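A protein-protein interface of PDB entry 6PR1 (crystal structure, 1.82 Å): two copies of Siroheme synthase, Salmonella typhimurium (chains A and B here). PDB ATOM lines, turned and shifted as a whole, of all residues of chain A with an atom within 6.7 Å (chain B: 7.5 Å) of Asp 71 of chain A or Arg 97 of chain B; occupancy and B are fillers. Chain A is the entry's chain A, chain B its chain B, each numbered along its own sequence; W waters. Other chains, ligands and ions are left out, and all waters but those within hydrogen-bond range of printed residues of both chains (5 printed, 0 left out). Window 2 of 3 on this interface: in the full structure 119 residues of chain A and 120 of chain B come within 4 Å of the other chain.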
ATOM      1  N   ASP A  14      -8.131 -15.525 -26.869  1.00  0.00           N
ATOM      2  CA  ASP A  14      -7.818 -15.578 -28.294  1.00  0.00           C
ATOM      3  C   ASP A  14      -7.206 -14.267 -28.763  1.00  0.00           C
ATOM      4  O   ASP A  14      -7.745 -13.190 -28.491  1.00  0.00           O
ATOM      5  CB  ASP A  14      -9.088 -15.849 -29.106  1.00  0.00           C
ATOM      6  CG  ASP A  14      -9.660 -17.239 -28.884  1.00  0.00           C
ATOM      7  OD1 ASP A  14      -8.978 -18.095 -28.287  1.00  0.00           O
ATOM      8  OD2 ASP A  14     -10.804 -17.471 -29.329  1.00  0.00           O
ATOM      9  N   GLU A  67     -11.286 -11.869 -42.105  1.00  0.00           N
ATOM     10  CA  GLU A  67     -11.651 -11.025 -40.974  1.00  0.00           C
ATOM     11  C   GLU A  67     -12.501 -11.772 -39.943  1.00  0.00           C
ATOM     12  O   GLU A  67     -12.573 -11.333 -38.795  1.00  0.00           O
ATOM     13  CB  GLU A  67     -12.385  -9.766 -41.445  1.00  0.00           C
ATOM     14  CG  GLU A  67     -13.788 -10.018 -41.896  1.00  0.00           C
ATOM     15  CD  GLU A  67     -14.538  -8.735 -42.192  1.00  0.00           C
ATOM     16  OE1 GLU A  67     -14.418  -8.230 -43.330  1.00  0.00           O
ATOM     17  OE2 GLU A  67     -15.242  -8.234 -41.286  1.00  0.00           O
ATOM     18  N   THR A  68     -13.139 -12.886 -40.314  1.00  0.00           N
ATOM     19  CA  THR A  68     -13.887 -13.627 -39.296  1.00  0.00           C
ATOM     20  C   THR A  68     -12.980 -14.214 -38.225  1.00  0.00           C
ATOM     21  O   THR A  68     -13.476 -14.580 -37.150  1.00  0.00           O
ATOM     22  CB  THR A  68     -14.760 -14.740 -39.913  1.00  0.00           C
ATOM     23  OG1 THR A  68     -13.957 -15.794 -40.465  1.00  0.00           O
ATOM     24  CG2 THR A  68     -15.685 -14.174 -40.997  1.00  0.00           C
ATOM     25  N   LEU A  69     -11.665 -14.297 -38.473  1.00  0.00           N
ATOM     26  CA  LEU A  69     -10.752 -14.776 -37.438  1.00  0.00           C
ATOM     27  C   LEU A  69     -10.656 -13.794 -36.281  1.00  0.00           C
ATOM     28  O   LEU A  69     -10.178 -14.161 -35.203  1.00  0.00           O
ATOM     29  CB  LEU A  69      -9.354 -15.023 -38.016  1.00  0.00           C
ATOM     30  CG  LEU A  69      -9.216 -16.196 -38.990  1.00  0.00           C
ATOM     31  CD1 LEU A  69      -7.836 -16.187 -39.631  1.00  0.00           C
ATOM     32  CD2 LEU A  69      -9.450 -17.495 -38.238  1.00  0.00           C
ATOM     33  N   LEU A  70     -11.117 -12.558 -36.469  1.00  0.00           N
ATOM     34  CA  LEU A  70     -11.167 -11.617 -35.357  1.00  0.00           C
ATOM     35  C   LEU A  70     -12.348 -11.847 -34.425  1.00  0.00           C
ATOM     36  O   LEU A  70     -12.370 -11.280 -33.328  1.00  0.00           O
ATOM     37  CB  LEU A  70     -11.240 -10.187 -35.883  1.00  0.00           C
ATOM     38  CG  LEU A  70      -9.928  -9.760 -36.541  1.00  0.00           C
ATOM     39  CD1 LEU A  70     -10.191  -8.515 -37.360  1.00  0.00           C
ATOM     40  CD2 LEU A  70      -8.908  -9.479 -35.476  1.00  0.00           C
ATOM     41  N   ASP A  71     -13.326 -12.664 -34.822  1.00  0.00           N
ATOM     42  CA  ASP A  71     -14.612 -12.623 -34.139  1.00  0.00           C
ATOM     43  C   ASP A  71     -14.511 -12.949 -32.659  1.00  0.00           C
ATOM     44  O   ASP A  71     -15.298 -12.422 -31.862  1.00  0.00           O
ATOM     45  CB  ASP A  71     -15.587 -13.552 -34.836  1.00  0.00           C
ATOM     46  CG  ASP A  71     -16.046 -12.982 -36.154  1.00  0.00           C
ATOM     47  OD1 ASP A  71     -15.647 -11.827 -36.449  1.00  0.00           O
ATOM     48  OD2 ASP A  71     -16.783 -13.663 -36.887  1.00  0.00           O
ATOM     49  N   SER A  72     -13.573 -13.798 -32.260  1.00  0.00           N
ATOM     50  CA  SER A  72     -13.460 -14.156 -30.848  1.00  0.00           C
ATOM     51  C   SER A  72     -12.278 -13.493 -30.151  1.00  0.00           C
ATOM     52  O   SER A  72     -11.926 -13.900 -29.035  1.00  0.00           O
ATOM     53  CB  SER A  72     -13.356 -15.674 -30.681  1.00  0.00           C
ATOM     54  OG  SER A  72     -12.099 -16.147 -31.144  1.00  0.00           O
ATOM     55  N   CYS A  73     -11.670 -12.478 -30.752  1.00  0.00           N
ATOM     56  CA  CYS A  73     -10.353 -12.039 -30.312  1.00  0.00           C
ATOM     57  C   CYS A  73     -10.423 -10.870 -29.343  1.00  0.00           C
ATOM     58  O   CYS A  73     -11.353 -10.058 -29.370  1.00  0.00           O
ATOM     59  CB  CYS A  73      -9.478 -11.655 -31.501  1.00  0.00           C
ATOM     60  SG  CYS A  73      -8.843 -13.114 -32.344  1.00  0.00           S
ATOM     61  N   TRP A  74      -9.385 -10.785 -28.509  1.00  0.00           N
ATOM     62  CA  TRP A  74      -9.163  -9.716 -27.546  1.00  0.00           C
ATOM     63  C   TRP A  74      -8.095  -8.724 -27.991  1.00  0.00           C
ATOM     64  O   TRP A  74      -8.115  -7.565 -27.559  1.00  0.00           O
ATOM     65  CB  TRP A  74      -8.740 -10.318 -26.204  1.00  0.00           C
ATOM     66  CG  TRP A  74      -9.768 -11.126 -25.494  1.00  0.00           C
ATOM     67  CD1 TRP A  74     -10.232 -12.378 -25.835  1.00  0.00           C
ATOM     68  CD2 TRP A  74     -10.425 -10.767 -24.279  1.00  0.00           C
ATOM     69  NE1 TRP A  74     -11.154 -12.804 -24.893  1.00  0.00           N
ATOM     70  CE2 TRP A  74     -11.288 -11.831 -23.932  1.00  0.00           C
ATOM     71  CE3 TRP A  74     -10.372  -9.640 -23.443  1.00  0.00           C
ATOM     72  CZ2 TRP A  74     -12.100 -11.795 -22.800  1.00  0.00           C
ATOM     73  CZ3 TRP A  74     -11.179  -9.608 -22.307  1.00  0.00           C
ATOM     74  CH2 TRP A  74     -12.030 -10.689 -21.994  1.00  0.00           C
ATOM     75  N   ARG A  96     -14.950  -4.103 -34.427  1.00  0.00           N
ATOM     76  CA  ARG A  96     -15.252  -5.058 -33.358  1.00  0.00           C
ATOM     77  C   ARG A  96     -14.803  -4.570 -31.989  1.00  0.00           C
ATOM     78  O   ARG A  96     -14.916  -5.322 -31.012  1.00  0.00           O
ATOM     79  CB  ARG A  96     -14.589  -6.417 -33.646  1.00  0.00           C
ATOM     80  CG  ARG A  96     -15.176  -7.151 -34.886  1.00  0.00           C
ATOM     81  CD  ARG A  96     -14.227  -8.273 -35.348  1.00  0.00           C
ATOM     82  NE  ARG A  96     -14.825  -9.107 -36.402  1.00  0.00           N
ATOM     83  CZ  ARG A  96     -15.013  -8.715 -37.658  1.00  0.00           C
ATOM     84  NH1 ARG A  96     -14.638  -7.500 -38.039  1.00  0.00           N
ATOM     85  NH2 ARG A  96     -15.561  -9.544 -38.545  1.00  0.00           N
ATOM     86  N   ARG A  97     -14.295  -3.340 -31.895  1.00  0.00           N
ATOM     87  CA  ARG A  97     -13.715  -2.801 -30.657  1.00  0.00           C
ATOM     88  C   ARG A  97     -12.628  -3.727 -30.077  1.00  0.00           C
ATOM     89  O   ARG A  97     -12.539  -3.970 -28.865  1.00  0.00           O
ATOM     90  CB  ARG A  97     -14.819  -2.500 -29.633  1.00  0.00           C
ATOM     91  CG  ARG A  97     -15.858  -1.479 -30.172  1.00  0.00           C
ATOM     92  CD  ARG A  97     -17.093  -1.392 -29.287  1.00  0.00           C
ATOM     93  NE  ARG A  97     -17.720  -2.701 -29.159  1.00  0.00           N
ATOM     94  CZ  ARG A  97     -18.553  -3.214 -30.054  1.00  0.00           C
ATOM     95  NH1 ARG A  97     -18.880  -2.521 -31.142  1.00  0.00           N
ATOM     96  NH2 ARG A  97     -19.054  -4.419 -29.862  1.00  0.00           N
ATOM     97  N   ILE A  98     -11.744  -4.198 -30.959  1.00  0.00           N
ATOM     98  CA  ILE A  98     -10.586  -5.006 -30.583  1.00  0.00           C
ATOM     99  C   ILE A  98      -9.353  -4.119 -30.675  1.00  0.00           C
ATOM    100  O   ILE A  98      -9.068  -3.561 -31.745  1.00  0.00           O
ATOM    101  CB  ILE A  98     -10.449  -6.237 -31.499  1.00  0.00           C
ATOM    102  CG1 ILE A  98     -11.704  -7.100 -31.384  1.00  0.00           C
ATOM    103  CG2 ILE A  98      -9.172  -7.040 -31.182  1.00  0.00           C
ATOM    104  CD1 ILE A  98     -11.826  -8.156 -32.529  1.00  0.00           C
ATOM    105  N   CYS B  73     -18.312  -0.373 -25.600  1.00  0.00           N
ATOM    106  CA  CYS B  73     -17.168   0.019 -24.790  1.00  0.00           C
ATOM    107  C   CYS B  73     -15.905  -0.759 -25.144  1.00  0.00           C
ATOM    108  O   CYS B  73     -15.951  -1.930 -25.534  1.00  0.00           O
ATOM    109  CB  CYS B  73     -17.465  -0.170 -23.305  1.00  0.00           C
ATOM    110  SG  CYS B  73     -18.433   1.166 -22.648  1.00  0.00           S
ATOM    111  N   TRP B  74     -14.767  -0.089 -24.960  1.00  0.00           N
ATOM    112  CA  TRP B  74     -13.426  -0.638 -25.183  1.00  0.00           C
ATOM    113  C   TRP B  74     -12.700  -1.028 -23.896  1.00  0.00           C
ATOM    114  O   TRP B  74     -11.799  -1.868 -23.930  1.00  0.00           O
ATOM    115  CB  TRP B  74     -12.548   0.386 -25.906  1.00  0.00           C
ATOM    116  CG  TRP B  74     -12.938   0.709 -27.327  1.00  0.00           C
ATOM    117  CD1 TRP B  74     -14.019   1.435 -27.747  1.00  0.00           C
ATOM    118  CD2 TRP B  74     -12.210   0.347 -28.504  1.00  0.00           C
ATOM    119  NE1 TRP B  74     -14.021   1.523 -29.129  1.00  0.00           N
ATOM    120  CE2 TRP B  74     -12.908   0.878 -29.612  1.00  0.00           C
ATOM    121  CE3 TRP B  74     -11.021  -0.371 -28.728  1.00  0.00           C
ATOM    122  CZ2 TRP B  74     -12.469   0.694 -30.934  1.00  0.00           C
ATOM    123  CZ3 TRP B  74     -10.575  -0.539 -30.038  1.00  0.00           C
ATOM    124  CH2 TRP B  74     -11.302  -0.010 -31.128  1.00  0.00           C
ATOM    125  N   ASP B  91     -18.055  -9.924 -15.087  1.00  0.00           N
ATOM    126  CA  ASP B  91     -18.616 -11.012 -15.885  1.00  0.00           C
ATOM    127  C   ASP B  91     -19.197 -10.504 -17.197  1.00  0.00           C
ATOM    128  O   ASP B  91     -19.050 -11.155 -18.240  1.00  0.00           O
ATOM    129  CB  ASP B  91     -19.695 -11.759 -15.094  1.00  0.00           C
ATOM    130  CG  ASP B  91     -19.126 -12.570 -13.930  1.00  0.00           C
ATOM    131  OD1 ASP B  91     -17.913 -12.860 -13.935  1.00  0.00           O
ATOM    132  OD2 ASP B  91     -19.906 -12.928 -13.017  1.00  0.00           O
ATOM    133  N   ALA B  92     -19.879  -9.358 -17.155  1.00  0.00           N
ATOM    134  CA  ALA B  92     -20.468  -8.790 -18.360  1.00  0.00           C
ATOM    135  C   ALA B  92     -19.387  -8.351 -19.336  1.00  0.00           C
ATOM    136  O   ALA B  92     -19.520  -8.550 -20.550  1.00  0.00           O
ATOM    137  CB  ALA B  92     -21.364  -7.614 -17.988  1.00  0.00           C
ATOM    138  N   ALA B  93     -18.313  -7.747 -18.821  1.00  0.00           N
ATOM    139  CA  ALA B  93     -17.220  -7.329 -19.694  1.00  0.00           C
ATOM    140  C   ALA B  93     -16.537  -8.535 -20.323  1.00  0.00           C
ATOM    141  O   ALA B  93     -16.203  -8.524 -21.516  1.00  0.00           O
ATOM    142  CB  ALA B  93     -16.208  -6.491 -18.905  1.00  0.00           C
ATOM    143  N   GLU B  94     -16.330  -9.590 -19.538  1.00  0.00           N
ATOM    144  CA  GLU B  94     -15.665 -10.784 -20.063  1.00  0.00           C
ATOM    145  C   GLU B  94     -16.461 -11.423 -21.200  1.00  0.00           C
ATOM    146  O   GLU B  94     -15.886 -11.836 -22.218  1.00  0.00           O
ATOM    147  CB  GLU B  94     -15.459 -11.786 -18.929  1.00  0.00           C
ATOM    148  CG  GLU B  94     -15.070 -13.176 -19.391  1.00  0.00           C
ATOM    149  CD  GLU B  94     -13.606 -13.457 -19.169  1.00  0.00           C
ATOM    150  OE1 GLU B  94     -13.211 -14.644 -19.209  1.00  0.00           O
ATOM    151  OE2 GLU B  94     -12.845 -12.488 -18.957  1.00  0.00           O
ATOM    152  N   SER B  95     -17.782 -11.524 -21.044  1.00  0.00           N
ATOM    153  CA  SER B  95     -18.612 -12.086 -22.108  1.00  0.00           C
ATOM    154  C   SER B  95     -18.530 -11.265 -23.394  1.00  0.00           C
ATOM    155  O   SER B  95     -18.731 -11.817 -24.483  1.00  0.00           O
ATOM    156  CB  SER B  95     -20.065 -12.211 -21.635  1.00  0.00           C
ATOM    157  OG  SER B  95     -20.697 -10.947 -21.554  1.00  0.00           O
ATOM    158  N   ARG B  96     -18.194  -9.981 -23.294  1.00  0.00           N
ATOM    159  CA  ARG B  96     -18.073  -9.076 -24.429  1.00  0.00           C
ATOM    160  C   ARG B  96     -16.630  -8.896 -24.909  1.00  0.00           C
ATOM    161  O   ARG B  96     -16.393  -8.090 -25.821  1.00  0.00           O
ATOM    162  CB  ARG B  96     -18.665  -7.705 -24.062  1.00  0.00           C
ATOM    163  CG  ARG B  96     -20.189  -7.677 -23.976  1.00  0.00           C
ATOM    164  CD  ARG B  96     -20.689  -6.382 -23.315  1.00  0.00           C
ATOM    165  NE  ARG B  96     -22.159  -6.308 -23.269  1.00  0.00           N
ATOM    166  CZ  ARG B  96     -22.920  -7.013 -22.437  1.00  0.00           C
ATOM    167  NH1 ARG B  96     -22.360  -7.844 -21.560  1.00  0.00           N
ATOM    168  NH2 ARG B  96     -24.246  -6.885 -22.479  1.00  0.00           N
ATOM    169  N   ARG B  97     -15.672  -9.628 -24.329  1.00  0.00           N
ATOM    170  CA  ARG B  97     -14.242  -9.490 -24.638  1.00  0.00           C
ATOM    171  C   ARG B  97     -13.767  -8.047 -24.463  1.00  0.00           C
ATOM    172  O   ARG B  97     -12.994  -7.515 -25.265  1.00  0.00           O
ATOM    173  CB  ARG B  97     -13.936 -10.027 -26.043  1.00  0.00           C
ATOM    174  CG  ARG B  97     -14.285 -11.515 -26.148  1.00  0.00           C
ATOM    175  CD  ARG B  97     -14.352 -12.039 -27.583  1.00  0.00           C
ATOM    176  NE  ARG B  97     -15.214 -11.223 -28.432  1.00  0.00           N
ATOM    177  CZ  ARG B  97     -16.529 -11.362 -28.563  1.00  0.00           C
ATOM    178  NH1 ARG B  97     -17.192 -12.307 -27.892  1.00  0.00           N
ATOM    179  NH2 ARG B  97     -17.185 -10.541 -29.373  1.00  0.00           N
ATOM    180  N   ILE B  98     -14.222  -7.408 -23.388  1.00  0.00           N
ATOM    181  CA  ILE B  98     -13.804  -6.057 -23.029  1.00  0.00           C
ATOM    182  C   ILE B  98     -12.819  -6.149 -21.869  1.00  0.00           C
ATOM    183  O   ILE B  98     -13.169  -6.654 -20.798  1.00  0.00           O
ATOM    184  CB  ILE B  98     -15.011  -5.192 -22.622  1.00  0.00           C
ATOM    185  CG1 ILE B  98     -15.992  -5.014 -23.791  1.00  0.00           C
ATOM    186  CG2 ILE B  98     -14.536  -3.873 -22.027  1.00  0.00           C
ATOM    187  CD1 ILE B  98     -17.304  -4.316 -23.369  1.00  0.00           C
ATOM    188  N   PHE B  99     -11.605  -5.626 -22.049  1.00  0.00           N
ATOM    189  CA  PHE B  99     -10.660  -5.638 -20.943  1.00  0.00           C
ATOM    190  C   PHE B  99     -11.236  -4.874 -19.761  1.00  0.00           C
ATOM    191  O   PHE B  99     -11.819  -3.798 -19.923  1.00  0.00           O
ATOM    192  CB  PHE B  99      -9.308  -5.060 -21.369  1.00  0.00           C
ATOM    193  CG  PHE B  99      -8.472  -6.045 -22.145  1.00  0.00           C
ATOM    194  CD1 PHE B  99      -7.960  -7.186 -21.524  1.00  0.00           C
ATOM    195  CD2 PHE B  99      -8.255  -5.876 -23.508  1.00  0.00           C
ATOM    196  CE1 PHE B  99      -7.205  -8.127 -22.258  1.00  0.00           C
ATOM    197  CE2 PHE B  99      -7.514  -6.802 -24.231  1.00  0.00           C
ATOM    198  CZ  PHE B  99      -6.998  -7.942 -23.602  1.00  0.00           C
ATOM    199  N   CYS B 100     -11.101  -5.457 -18.578  1.00  0.00           N
ATOM    200  CA  CYS B 100     -11.789  -4.958 -17.396  1.00  0.00           C
ATOM    201  C   CYS B 100     -10.851  -5.031 -16.195  1.00  0.00           C
ATOM    202  O   CYS B 100     -10.125  -6.014 -16.026  1.00  0.00           O
ATOM    203  CB  CYS B 100     -13.052  -5.785 -17.146  1.00  0.00           C
ATOM    204  SG  CYS B 100     -14.023  -5.205 -15.712  1.00  0.00           S
ATOM    205  N   SER B 110      -9.365  -8.731 -16.126  1.00  0.00           N
ATOM    206  CA  SER B 110      -8.515  -9.012 -17.272  1.00  0.00           C
ATOM    207  C   SER B 110      -7.438  -7.963 -17.526  1.00  0.00           C
ATOM    208  O   SER B 110      -6.597  -8.178 -18.407  1.00  0.00           O
ATOM    209  CB  SER B 110      -9.390  -9.205 -18.525  1.00  0.00           C
ATOM    210  OG  SER B 110     -10.255  -8.097 -18.704  1.00  0.00           O
HETATM  211  O   HOH W   1     -13.987  -9.275 -29.960  1.00  0.00           O
HETATM  212  O   HOH W   2     -13.847  -4.173 -26.491  1.00  0.00           O
HETATM  213  O   HOH W   3     -12.071  -7.330 -27.768  1.00  0.00           O
HETATM  214  O   HOH W   4     -15.546  -9.766 -32.365  1.00  0.00           O
HETATM  215  O   HOH W   5     -17.183  -3.974 -26.941  1.00  0.00           O
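Asp 71 of chain A touches just one residue of chain B: Arg 97.
Printed residues of chain A within 4 Å of Arg 97 of chain B: Asp 71 (3.6 Å), Ser 72 (3.4 Å) and Trp 74 (3.6 Å).
Printed residues of chain A within 4 Å of Cys 73 of chain B: Arg 97 (3.96 Å).
Printed residues of chain B within 4 Å of Arg 97 of chain A: Cys 73 and Trp 74.
Ala 92 of chain B touches none of the printed residues of chain A.
The nearest printed residue of chain B that does not touch Arg 97 of chain A is Arg 97 of chain B (5.1 Å).
Among the printed residues, pairs that only touch across the chains: Asp 71 of chain A with Arg 97 of chain B (3.6 Å), Ser 72 of chain A with Arg 97 of chain B (3.4 Å), Trp 74 of chain A with Glu 94 of chain B (3.6 Å), Trp 74 of chain A with Arg 97 of chain B (3.6 Å), Trp 74 of chain A with Ile 98 of chain B (3.9 Å), Trp 74 of chain A with Phe 99 of chain B (3.5 Å), Arg 97 of chain A with Cys 73 of chain B (3.96 Å), Arg 97 of chain A with Trp 74 of chain B (3.7 Å) and Ile 98 of chain A with Trp 74 of chain B (3.8 Å).
Water W5 bridges NE of Arg 97 of chain A (2.6 Å) and O of Cys 73 of chain B (2.8 Å).
Water W3 bridges the backbone carbonyl oxygen (O) of Arg 97 of chain B (2.7 Å) and the backbone carbonyl oxygen (O) of Cys 73 of chain A (3.2 Å).
Water W4 bridges O of Asp 71 of chain A (2.7 Å) and NH2 of Arg 97 of chain B (3.5 Å).
Water W2 bridges the backbone carbonyl oxygen (O) of Arg 97 of chain A (2.7 Å) and the backbone carbonyl oxygen (O) of Cys 73 of chain B (3.2 Å).
Water W1 bridges NE of Arg 97 of chain B (2.8 Å) and O of Cys 73 of chain A (2.8 Å).
NE of Arg 96 of chain A lies within salt-bridge range of OD1 of Asp 71 of chain A (2.8 Å).
N of Ile 98 of chain B is in hydrogen-bond range of O of Ala 93 of chain B (2.9 Å).
OD2 of Asp 14 of chain A lies within hydrogen-bond range of OG of Ser 72 of chain A.
The backbone carbonyl oxygen (O) of Asp 14 of chain A is in hydrogen-bond range of the backbone NH (N) of Trp 74 of chain A, 2.9 Å away.
Of the 12 printed residues of chain A, 5 touch a printed residue of chain B.
Printed residues of chain A that touch a printed residue of chain B: Asp 71, Ser 72, Trp 74, Arg 97 and Ile 98.
Hydrophobic or aromatic side chains of chain A that line the printed part of chain B: Trp 74.
Of the 13 printed residues of chain B, 6 touch a printed residue of chain A.
Among the printed residues, no Asp or Glu carboxylate lies within 4 Å of a Lys or Arg side-chain nitrogen of the other chain.
Trp 74 of chain A touches Arg 97 of chain B, and with the chains exchanged Arg 97 of chain A touches Trp 74 of chain B.
Trp 74 of chain A touches Ile 98 of chain B, and with the chains exchanged Ile 98 of chain A touches Trp 74 of chain B.
Arg 97 of chain A touches Cys 73 of chain B, but with the chains exchanged Cys 73 of chain A does not touch Arg 97 of chain B (4.01 Å).
Positions printed for both chains: 73, 74, 96, 97 and 98.
Of the 9 pairs that touch across the chains among the printed residues, 4 have their exchanged pair printed and touching as well.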
